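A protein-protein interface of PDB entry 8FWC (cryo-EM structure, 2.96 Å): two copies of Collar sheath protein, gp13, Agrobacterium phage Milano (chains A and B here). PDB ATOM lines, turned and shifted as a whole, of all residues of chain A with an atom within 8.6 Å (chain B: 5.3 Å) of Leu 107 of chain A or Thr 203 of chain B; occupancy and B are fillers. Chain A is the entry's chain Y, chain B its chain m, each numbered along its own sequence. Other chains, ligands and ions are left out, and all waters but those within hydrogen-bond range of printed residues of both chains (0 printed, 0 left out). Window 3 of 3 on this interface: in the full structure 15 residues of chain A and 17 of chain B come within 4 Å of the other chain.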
ATOM      1  N   ARG A  30     -26.143 -29.544  11.124  1.00  0.00           N
ATOM      2  CA  ARG A  30     -25.755 -29.094  12.445  1.00  0.00           C
ATOM      3  C   ARG A  30     -25.948 -30.213  13.459  1.00  0.00           C
ATOM      4  O   ARG A  30     -26.980 -30.885  13.438  1.00  0.00           O
ATOM      5  CB  ARG A  30     -26.579 -27.873  12.858  1.00  0.00           C
ATOM      6  CG  ARG A  30     -26.633 -27.635  14.345  1.00  0.00           C
ATOM      7  CD  ARG A  30     -27.037 -26.213  14.663  1.00  0.00           C
ATOM      8  NE  ARG A  30     -26.642 -25.840  16.016  1.00  0.00           N
ATOM      9  CZ  ARG A  30     -26.657 -24.597  16.481  1.00  0.00           C
ATOM     10  NH1 ARG A  30     -27.051 -23.602  15.703  1.00  0.00           N
ATOM     11  NH2 ARG A  30     -26.277 -24.349  17.725  1.00  0.00           N
ATOM     12  N   PRO A  31     -24.984 -30.442  14.348  1.00  0.00           N
ATOM     13  CA  PRO A  31     -25.076 -31.586  15.262  1.00  0.00           C
ATOM     14  C   PRO A  31     -26.297 -31.543  16.158  1.00  0.00           C
ATOM     15  O   PRO A  31     -26.511 -30.569  16.881  1.00  0.00           O
ATOM     16  CB  PRO A  31     -23.787 -31.479  16.081  1.00  0.00           C
ATOM     17  CG  PRO A  31     -22.879 -30.683  15.250  1.00  0.00           C
ATOM     18  CD  PRO A  31     -23.730 -29.702  14.532  1.00  0.00           C
ATOM     19  N   GLY A  32     -27.105 -32.594  16.116  1.00  0.00           N
ATOM     20  CA  GLY A  32     -28.313 -32.693  16.907  1.00  0.00           C
ATOM     21  C   GLY A  32     -29.586 -32.538  16.108  1.00  0.00           C
ATOM     22  O   GLY A  32     -30.641 -33.007  16.549  1.00  0.00           O
ATOM     23  N   ILE A 104     -23.423 -33.447  31.497  1.00  0.00           N
ATOM     24  CA  ILE A 104     -24.584 -34.052  30.858  1.00  0.00           C
ATOM     25  C   ILE A 104     -25.457 -32.909  30.362  1.00  0.00           C
ATOM     26  O   ILE A 104     -26.120 -32.232  31.152  1.00  0.00           O
ATOM     27  CB  ILE A 104     -25.359 -34.967  31.808  1.00  0.00           C
ATOM     28  CG1 ILE A 104     -24.413 -35.922  32.528  1.00  0.00           C
ATOM     29  CG2 ILE A 104     -26.401 -35.746  31.040  1.00  0.00           C
ATOM     30  CD1 ILE A 104     -24.015 -37.102  31.703  1.00  0.00           C
ATOM     31  N   SER A 105     -25.464 -32.687  29.055  1.00  0.00           N
ATOM     32  CA  SER A 105     -26.242 -31.602  28.466  1.00  0.00           C
ATOM     33  C   SER A 105     -27.732 -31.873  28.646  1.00  0.00           C
ATOM     34  O   SER A 105     -28.202 -32.995  28.421  1.00  0.00           O
ATOM     35  CB  SER A 105     -25.894 -31.458  26.991  1.00  0.00           C
ATOM     36  OG  SER A 105     -27.034 -31.653  26.181  1.00  0.00           O
ATOM     37  N   GLU A 106     -28.479 -30.848  29.061  1.00  0.00           N
ATOM     38  CA  GLU A 106     -29.919 -30.993  29.221  1.00  0.00           C
ATOM     39  C   GLU A 106     -30.660 -31.097  27.900  1.00  0.00           C
ATOM     40  O   GLU A 106     -31.808 -31.547  27.892  1.00  0.00           O
ATOM     41  CB  GLU A 106     -30.485 -29.800  29.992  1.00  0.00           C
ATOM     42  CG  GLU A 106     -30.093 -29.781  31.438  1.00  0.00           C
ATOM     43  CD  GLU A 106     -30.288 -28.427  32.072  1.00  0.00           C
ATOM     44  OE1 GLU A 106     -29.770 -27.435  31.528  1.00  0.00           O
ATOM     45  OE2 GLU A 106     -30.941 -28.361  33.137  1.00  0.00           O
ATOM     46  N   LEU A 107     -30.050 -30.678  26.794  1.00  0.00           N
ATOM     47  CA  LEU A 107     -30.716 -30.802  25.506  1.00  0.00           C
ATOM     48  C   LEU A 107     -30.763 -32.254  25.059  1.00  0.00           C
ATOM     49  O   LEU A 107     -31.693 -32.669  24.361  1.00  0.00           O
ATOM     50  CB  LEU A 107     -30.006 -29.948  24.465  1.00  0.00           C
ATOM     51  CG  LEU A 107     -30.134 -28.433  24.565  1.00  0.00           C
ATOM     52  CD1 LEU A 107     -29.747 -27.801  23.258  1.00  0.00           C
ATOM     53  CD2 LEU A 107     -31.525 -28.037  24.927  1.00  0.00           C
ATOM     54  N   ASN A 108     -29.762 -33.036  25.437  1.00  0.00           N
ATOM     55  CA  ASN A 108     -29.631 -34.417  25.004  1.00  0.00           C
ATOM     56  C   ASN A 108     -29.593 -35.365  26.191  1.00  0.00           C
ATOM     57  O   ASN A 108     -28.819 -36.319  26.219  1.00  0.00           O
ATOM     58  CB  ASN A 108     -28.388 -34.590  24.143  1.00  0.00           C
ATOM     59  CG  ASN A 108     -28.394 -33.690  22.937  1.00  0.00           C
ATOM     60  OD1 ASN A 108     -29.310 -33.736  22.119  1.00  0.00           O
ATOM     61  ND2 ASN A 108     -27.367 -32.867  22.814  1.00  0.00           N
ATOM     62  N   GLY A 109     -30.424 -35.111  27.193  1.00  0.00           N
ATOM     63  CA  GLY A 109     -30.495 -35.976  28.342  1.00  0.00           C
ATOM     64  C   GLY A 109     -31.216 -37.262  28.009  1.00  0.00           C
ATOM     65  O   GLY A 109     -31.514 -37.548  26.848  1.00  0.00           O
ATOM     66  N   PRO A 110     -31.516 -38.063  29.024  1.00  0.00           N
ATOM     67  CA  PRO A 110     -32.242 -39.312  28.779  1.00  0.00           C
ATOM     68  C   PRO A 110     -33.690 -39.060  28.410  1.00  0.00           C
ATOM     69  O   PRO A 110     -34.144 -37.914  28.413  1.00  0.00           O
ATOM     70  CB  PRO A 110     -32.120 -40.055  30.111  1.00  0.00           C
ATOM     71  CG  PRO A 110     -31.923 -38.991  31.109  1.00  0.00           C
ATOM     72  CD  PRO A 110     -31.137 -37.912  30.435  1.00  0.00           C
ATOM     73  N   SER A 111     -34.425 -40.117  28.101  1.00  0.00           N
ATOM     74  CA  SER A 111     -35.795 -39.981  27.629  1.00  0.00           C
ATOM     75  C   SER A 111     -36.821 -40.602  28.559  1.00  0.00           C
ATOM     76  O   SER A 111     -37.948 -40.109  28.637  1.00  0.00           O
ATOM     77  CB  SER A 111     -35.934 -40.602  26.236  1.00  0.00           C
ATOM     78  OG  SER A 111     -35.088 -39.951  25.307  1.00  0.00           O
ATOM     79  N   PHE A 137     -28.273 -41.254  26.569  1.00  0.00           N
ATOM     80  CA  PHE A 137     -27.997 -39.869  26.911  1.00  0.00           C
ATOM     81  C   PHE A 137     -26.579 -39.557  26.475  1.00  0.00           C
ATOM     82  O   PHE A 137     -25.733 -40.448  26.397  1.00  0.00           O
ATOM     83  CB  PHE A 137     -28.191 -39.584  28.403  1.00  0.00           C
ATOM     84  CG  PHE A 137     -27.212 -40.278  29.292  1.00  0.00           C
ATOM     85  CD1 PHE A 137     -27.456 -41.557  29.743  1.00  0.00           C
ATOM     86  CD2 PHE A 137     -26.060 -39.639  29.701  1.00  0.00           C
ATOM     87  CE1 PHE A 137     -26.562 -42.190  30.568  1.00  0.00           C
ATOM     88  CE2 PHE A 137     -25.164 -40.268  30.522  1.00  0.00           C
ATOM     89  CZ  PHE A 137     -25.415 -41.543  30.957  1.00  0.00           C
ATOM     90  N   TRP A 138     -26.336 -38.289  26.176  1.00  0.00           N
ATOM     91  CA  TRP A 138     -25.086 -37.854  25.576  1.00  0.00           C
ATOM     92  C   TRP A 138     -24.306 -37.009  26.570  1.00  0.00           C
ATOM     93  O   TRP A 138     -24.721 -35.897  26.904  1.00  0.00           O
ATOM     94  CB  TRP A 138     -25.359 -37.068  24.299  1.00  0.00           C
ATOM     95  CG  TRP A 138     -26.133 -37.855  23.318  1.00  0.00           C
ATOM     96  CD1 TRP A 138     -27.462 -38.128  23.356  1.00  0.00           C
ATOM     97  CD2 TRP A 138     -25.624 -38.491  22.152  1.00  0.00           C
ATOM     98  NE1 TRP A 138     -27.816 -38.895  22.280  1.00  0.00           N
ATOM     99  CE2 TRP A 138     -26.701 -39.131  21.524  1.00  0.00           C
ATOM    100  CE3 TRP A 138     -24.361 -38.580  21.574  1.00  0.00           C
ATOM    101  CZ2 TRP A 138     -26.553 -39.847  20.353  1.00  0.00           C
ATOM    102  CZ3 TRP A 138     -24.217 -39.290  20.415  1.00  0.00           C
ATOM    103  CH2 TRP A 138     -25.304 -39.913  19.814  1.00  0.00           C
ATOM    104  N   PRO A 192     -25.591 -35.884  17.954  1.00  0.00           N
ATOM    105  CA  PRO A 192     -24.939 -34.787  18.675  1.00  0.00           C
ATOM    106  C   PRO A 192     -23.437 -34.935  18.783  1.00  0.00           C
ATOM    107  O   PRO A 192     -22.770 -33.981  19.202  1.00  0.00           O
ATOM    108  CB  PRO A 192     -25.586 -34.847  20.062  1.00  0.00           C
ATOM    109  CG  PRO A 192     -26.820 -35.616  19.879  1.00  0.00           C
ATOM    110  CD  PRO A 192     -26.524 -36.612  18.821  1.00  0.00           C
ATOM    111  N   THR B  58     -36.981 -27.490  24.660  1.00  0.00           N
ATOM    112  CA  THR B  58     -36.018 -27.589  25.740  1.00  0.00           C
ATOM    113  C   THR B  58     -35.090 -26.389  25.678  1.00  0.00           C
ATOM    114  O   THR B  58     -34.623 -26.014  24.601  1.00  0.00           O
ATOM    115  CB  THR B  58     -35.223 -28.884  25.641  1.00  0.00           C
ATOM    116  OG1 THR B  58     -36.129 -29.986  25.551  1.00  0.00           O
ATOM    117  CG2 THR B  58     -34.374 -29.071  26.871  1.00  0.00           C
ATOM    118  N   PHE B  59     -34.833 -25.784  26.831  1.00  0.00           N
ATOM    119  CA  PHE B  59     -34.003 -24.596  26.926  1.00  0.00           C
ATOM    120  C   PHE B  59     -32.765 -24.894  27.755  1.00  0.00           C
ATOM    121  O   PHE B  59     -32.761 -25.802  28.586  1.00  0.00           O
ATOM    122  CB  PHE B  59     -34.765 -23.436  27.558  1.00  0.00           C
ATOM    123  CG  PHE B  59     -35.992 -23.039  26.806  1.00  0.00           C
ATOM    124  CD1 PHE B  59     -35.925 -22.106  25.799  1.00  0.00           C
ATOM    125  CD2 PHE B  59     -37.213 -23.591  27.111  1.00  0.00           C
ATOM    126  CE1 PHE B  59     -37.046 -21.739  25.111  1.00  0.00           C
ATOM    127  CE2 PHE B  59     -38.334 -23.221  26.420  1.00  0.00           C
ATOM    128  CZ  PHE B  59     -38.249 -22.297  25.422  1.00  0.00           C
ATOM    129  N   GLU B  60     -31.713 -24.118  27.527  1.00  0.00           N
ATOM    130  CA  GLU B  60     -30.514 -24.234  28.339  1.00  0.00           C
ATOM    131  C   GLU B  60     -29.835 -22.879  28.404  1.00  0.00           C
ATOM    132  O   GLU B  60     -29.675 -22.220  27.375  1.00  0.00           O
ATOM    133  CB  GLU B  60     -29.559 -25.276  27.770  1.00  0.00           C
ATOM    134  CG  GLU B  60     -28.363 -25.518  28.646  1.00  0.00           C
ATOM    135  CD  GLU B  60     -27.430 -26.553  28.076  1.00  0.00           C
ATOM    136  OE1 GLU B  60     -27.701 -27.046  26.963  1.00  0.00           O
ATOM    137  OE2 GLU B  60     -26.425 -26.878  28.742  1.00  0.00           O
ATOM    138  N   ILE B  61     -29.444 -22.467  29.604  1.00  0.00           N
ATOM    139  CA  ILE B  61     -28.761 -21.200  29.818  1.00  0.00           C
ATOM    140  C   ILE B  61     -27.324 -21.493  30.208  1.00  0.00           C
ATOM    141  O   ILE B  61     -27.065 -22.326  31.083  1.00  0.00           O
ATOM    142  CB  ILE B  61     -29.451 -20.350  30.899  1.00  0.00           C
ATOM    143  CG1 ILE B  61     -30.908 -20.090  30.539  1.00  0.00           C
ATOM    144  CG2 ILE B  61     -28.757 -19.023  31.030  1.00  0.00           C
ATOM    145  CD1 ILE B  61     -31.074 -19.221  29.341  1.00  0.00           C
ATOM    146  N   ARG B 201     -26.055 -17.242  27.113  1.00  0.00           N
ATOM    147  CA  ARG B 201     -26.434 -17.899  25.871  1.00  0.00           C
ATOM    148  C   ARG B 201     -27.587 -18.851  26.128  1.00  0.00           C
ATOM    149  O   ARG B 201     -27.498 -19.718  27.000  1.00  0.00           O
ATOM    150  CB  ARG B 201     -25.259 -18.659  25.269  1.00  0.00           C
ATOM    151  CG  ARG B 201     -25.640 -19.558  24.127  1.00  0.00           C
ATOM    152  CD  ARG B 201     -24.424 -19.955  23.343  1.00  0.00           C
ATOM    153  NE  ARG B 201     -23.808 -18.804  22.704  1.00  0.00           N
ATOM    154  CZ  ARG B 201     -22.535 -18.755  22.339  1.00  0.00           C
ATOM    155  NH1 ARG B 201     -21.747 -19.793  22.561  1.00  0.00           N
ATOM    156  NH2 ARG B 201     -22.048 -17.669  21.760  1.00  0.00           N
ATOM    157  N   LEU B 202     -28.657 -18.695  25.365  1.00  0.00           N
ATOM    158  CA  LEU B 202     -29.839 -19.534  25.473  1.00  0.00           C
ATOM    159  C   LEU B 202     -29.925 -20.402  24.231  1.00  0.00           C
ATOM    160  O   LEU B 202     -29.914 -19.882  23.116  1.00  0.00           O
ATOM    161  CB  LEU B 202     -31.093 -18.677  25.621  1.00  0.00           C
ATOM    162  CG  LEU B 202     -32.447 -19.297  25.296  1.00  0.00           C
ATOM    163  CD1 LEU B 202     -32.939 -20.143  26.434  1.00  0.00           C
ATOM    164  CD2 LEU B 202     -33.443 -18.211  24.986  1.00  0.00           C
ATOM    165  N   THR B 203     -30.012 -21.711  24.425  1.00  0.00           N
ATOM    166  CA  THR B 203     -30.168 -22.665  23.334  1.00  0.00           C
ATOM    167  C   THR B 203     -31.557 -23.278  23.386  1.00  0.00           C
ATOM    168  O   THR B 203     -31.997 -23.741  24.441  1.00  0.00           O
ATOM    169  CB  THR B 203     -29.110 -23.765  23.398  1.00  0.00           C
ATOM    170  OG1 THR B 203     -27.937 -23.266  24.058  1.00  0.00           O
ATOM    171  CG2 THR B 203     -28.750 -24.234  22.019  1.00  0.00           C
ATOM    172  N   VAL B 204     -32.239 -23.276  22.246  1.00  0.00           N
ATOM    173  CA  VAL B 204     -33.615 -23.739  22.127  1.00  0.00           C
ATOM    174  C   VAL B 204     -33.642 -24.929  21.184  1.00  0.00           C
ATOM    175  O   VAL B 204     -33.180 -24.828  20.045  1.00  0.00           O
ATOM    176  CB  VAL B 204     -34.529 -22.616  21.611  1.00  0.00           C
ATOM    177  CG1 VAL B 204     -35.958 -23.083  21.536  1.00  0.00           C
ATOM    178  CG2 VAL B 204     -34.413 -21.402  22.493  1.00  0.00           C
ATOM    179  N   ARG B 205     -34.183 -26.048  21.649  1.00  0.00           N
ATOM    180  CA  ARG B 205     -34.325 -27.251  20.841  1.00  0.00           C
ATOM    181  C   ARG B 205     -35.803 -27.539  20.648  1.00  0.00           C
ATOM    182  O   ARG B 205     -36.473 -27.995  21.576  1.00  0.00           O
ATOM    183  CB  ARG B 205     -33.636 -28.440  21.498  1.00  0.00           C
ATOM    184  CG  ARG B 205     -33.888 -29.757  20.803  1.00  0.00           C
ATOM    185  CD  ARG B 205     -33.301 -30.900  21.590  1.00  0.00           C
ATOM    186  NE  ARG B 205     -33.369 -32.164  20.872  1.00  0.00           N
ATOM    187  CZ  ARG B 205     -34.419 -32.971  20.889  1.00  0.00           C
ATOM    188  NH1 ARG B 205     -35.491 -32.642  21.586  1.00  0.00           N
ATOM    189  NH2 ARG B 205     -34.398 -34.106  20.212  1.00  0.00           N
ATOM    190  N   ILE B 219     -32.379 -26.649  16.214  1.00  0.00           N
ATOM    191  CA  ILE B 219     -31.615 -26.049  17.300  1.00  0.00           C
ATOM    192  C   ILE B 219     -31.131 -24.669  16.879  1.00  0.00           C
ATOM    193  O   ILE B 219     -30.670 -24.488  15.749  1.00  0.00           O
ATOM    194  CB  ILE B 219     -30.422 -26.926  17.710  1.00  0.00           C
ATOM    195  CG1 ILE B 219     -30.882 -28.351  17.984  1.00  0.00           C
ATOM    196  CG2 ILE B 219     -29.756 -26.360  18.937  1.00  0.00           C
ATOM    197  CD1 ILE B 219     -29.870 -29.175  18.711  1.00  0.00           C
ATOM    198  N   SER B 220     -31.239 -23.701  17.786  1.00  0.00           N
ATOM    199  CA  SER B 220     -30.724 -22.355  17.581  1.00  0.00           C
ATOM    200  C   SER B 220     -30.313 -21.780  18.928  1.00  0.00           C
ATOM    201  O   SER B 220     -30.627 -22.344  19.975  1.00  0.00           O
ATOM    202  CB  SER B 220     -31.758 -21.452  16.916  1.00  0.00           C
ATOM    203  OG  SER B 220     -32.956 -21.434  17.663  1.00  0.00           O
ATOM    204  N   CYS B 221     -29.602 -20.651  18.906  1.00  0.00           N
ATOM    205  CA  CYS B 221     -29.203 -20.013  20.152  1.00  0.00           C
ATOM    206  C   CYS B 221     -29.552 -18.539  20.110  1.00  0.00           C
ATOM    207  O   CYS B 221     -29.810 -17.976  19.047  1.00  0.00           O
ATOM    208  CB  CYS B 221     -27.719 -20.058  20.444  1.00  0.00           C
ATOM    209  SG  CYS B 221     -26.663 -20.545  19.143  1.00  0.00           S
ATOM    210  N   TYR B 222     -29.539 -17.919  21.285  1.00  0.00           N
ATOM    211  CA  TYR B 222     -29.666 -16.477  21.408  1.00  0.00           C
ATOM    212  C   TYR B 222     -28.695 -15.993  22.471  1.00  0.00           C
ATOM    213  O   TYR B 222     -28.489 -16.657  23.487  1.00  0.00           O
ATOM    214  CB  TYR B 222     -31.094 -16.069  21.755  1.00  0.00           C
ATOM    215  CG  TYR B 222     -32.101 -16.671  20.817  1.00  0.00           C
ATOM    216  CD1 TYR B 222     -32.479 -16.012  19.669  1.00  0.00           C
ATOM    217  CD2 TYR B 222     -32.659 -17.906  21.074  1.00  0.00           C
ATOM    218  CE1 TYR B 222     -33.382 -16.560  18.808  1.00  0.00           C
ATOM    219  CE2 TYR B 222     -33.563 -18.461  20.217  1.00  0.00           C
ATOM    220  CZ  TYR B 222     -33.921 -17.782  19.085  1.00  0.00           C
ATOM    221  OH  TYR B 222     -34.829 -18.330  18.218  1.00  0.00           O
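N of Leu 107 of chain A sits close to OG of Ser 105 of chain A (3.2 Å). O of Glu 60 of chain B lies within hydrogen-bond range of N of Thr 203 of chain B (3.0 Å). The backbone carbonyl oxygen (O) of Thr 58 of chain B lies within hydrogen-bond range of the backbone NH (N) of Arg 205 of chain B, 3.0 Å away.
Hydrophobic or aromatic side chains of chain A that line the printed part of chain B: Leu 107. Among the printed residues, 7 pairs touch across the chains.
Leu 107 of chain A touches just these residues of chain B: Thr 58 (3.6 Å), Glu 60 (3.7 Å), Thr 203 (3.9 Å) and Arg 205 (3.7 Å). Thr 203 of chain B touches just one residue of chain A: Leu 107. Of the printed residues of chain A, Glu 60 of chain B touches Glu 106 and Leu 107. Printed residues of chain A within 4 Å of Thr 58 of chain B: Glu 106 (3.7 Å) and Leu 107 (3.6 Å). Of the printed residues of chain B, Glu 106 of chain A touches Thr 58 (3.7 Å) and Glu 60 (3.7 Å). Of the printed residues of chain A, Ile 219 of chain B touches Arg 30 (3.7 Å). Pro 31 of chain A touches none of the printed residues of chain B. The nearest residue of chain B that does not touch Leu 107 of chain A is Phe 59 of chain B (4.4 Å). The nearest printed residue of chain B that does not touch Glu 106 of chain A is Phe 59 of chain B (4.5 Å).
No position is printed for both chains. Of the 7 pairs that touch across the chains among the printed residues, none has its exchanged pair printed and touching as well.
Among the printed residues, pairs that only touch across the chains: Arg 30 of chain A with Ile 219 of chain B, Glu 106 of chain A with Thr 58 of chain B, Glu 106 of chain A with Glu 60 of chain B, Leu 107 of chain A with Thr 58 of chain B, Leu 107 of chain A with Glu 60 of chain B, Leu 107 of chain A with Thr 203 of chain B and Leu 107 of chain A with Arg 205 of chain B.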
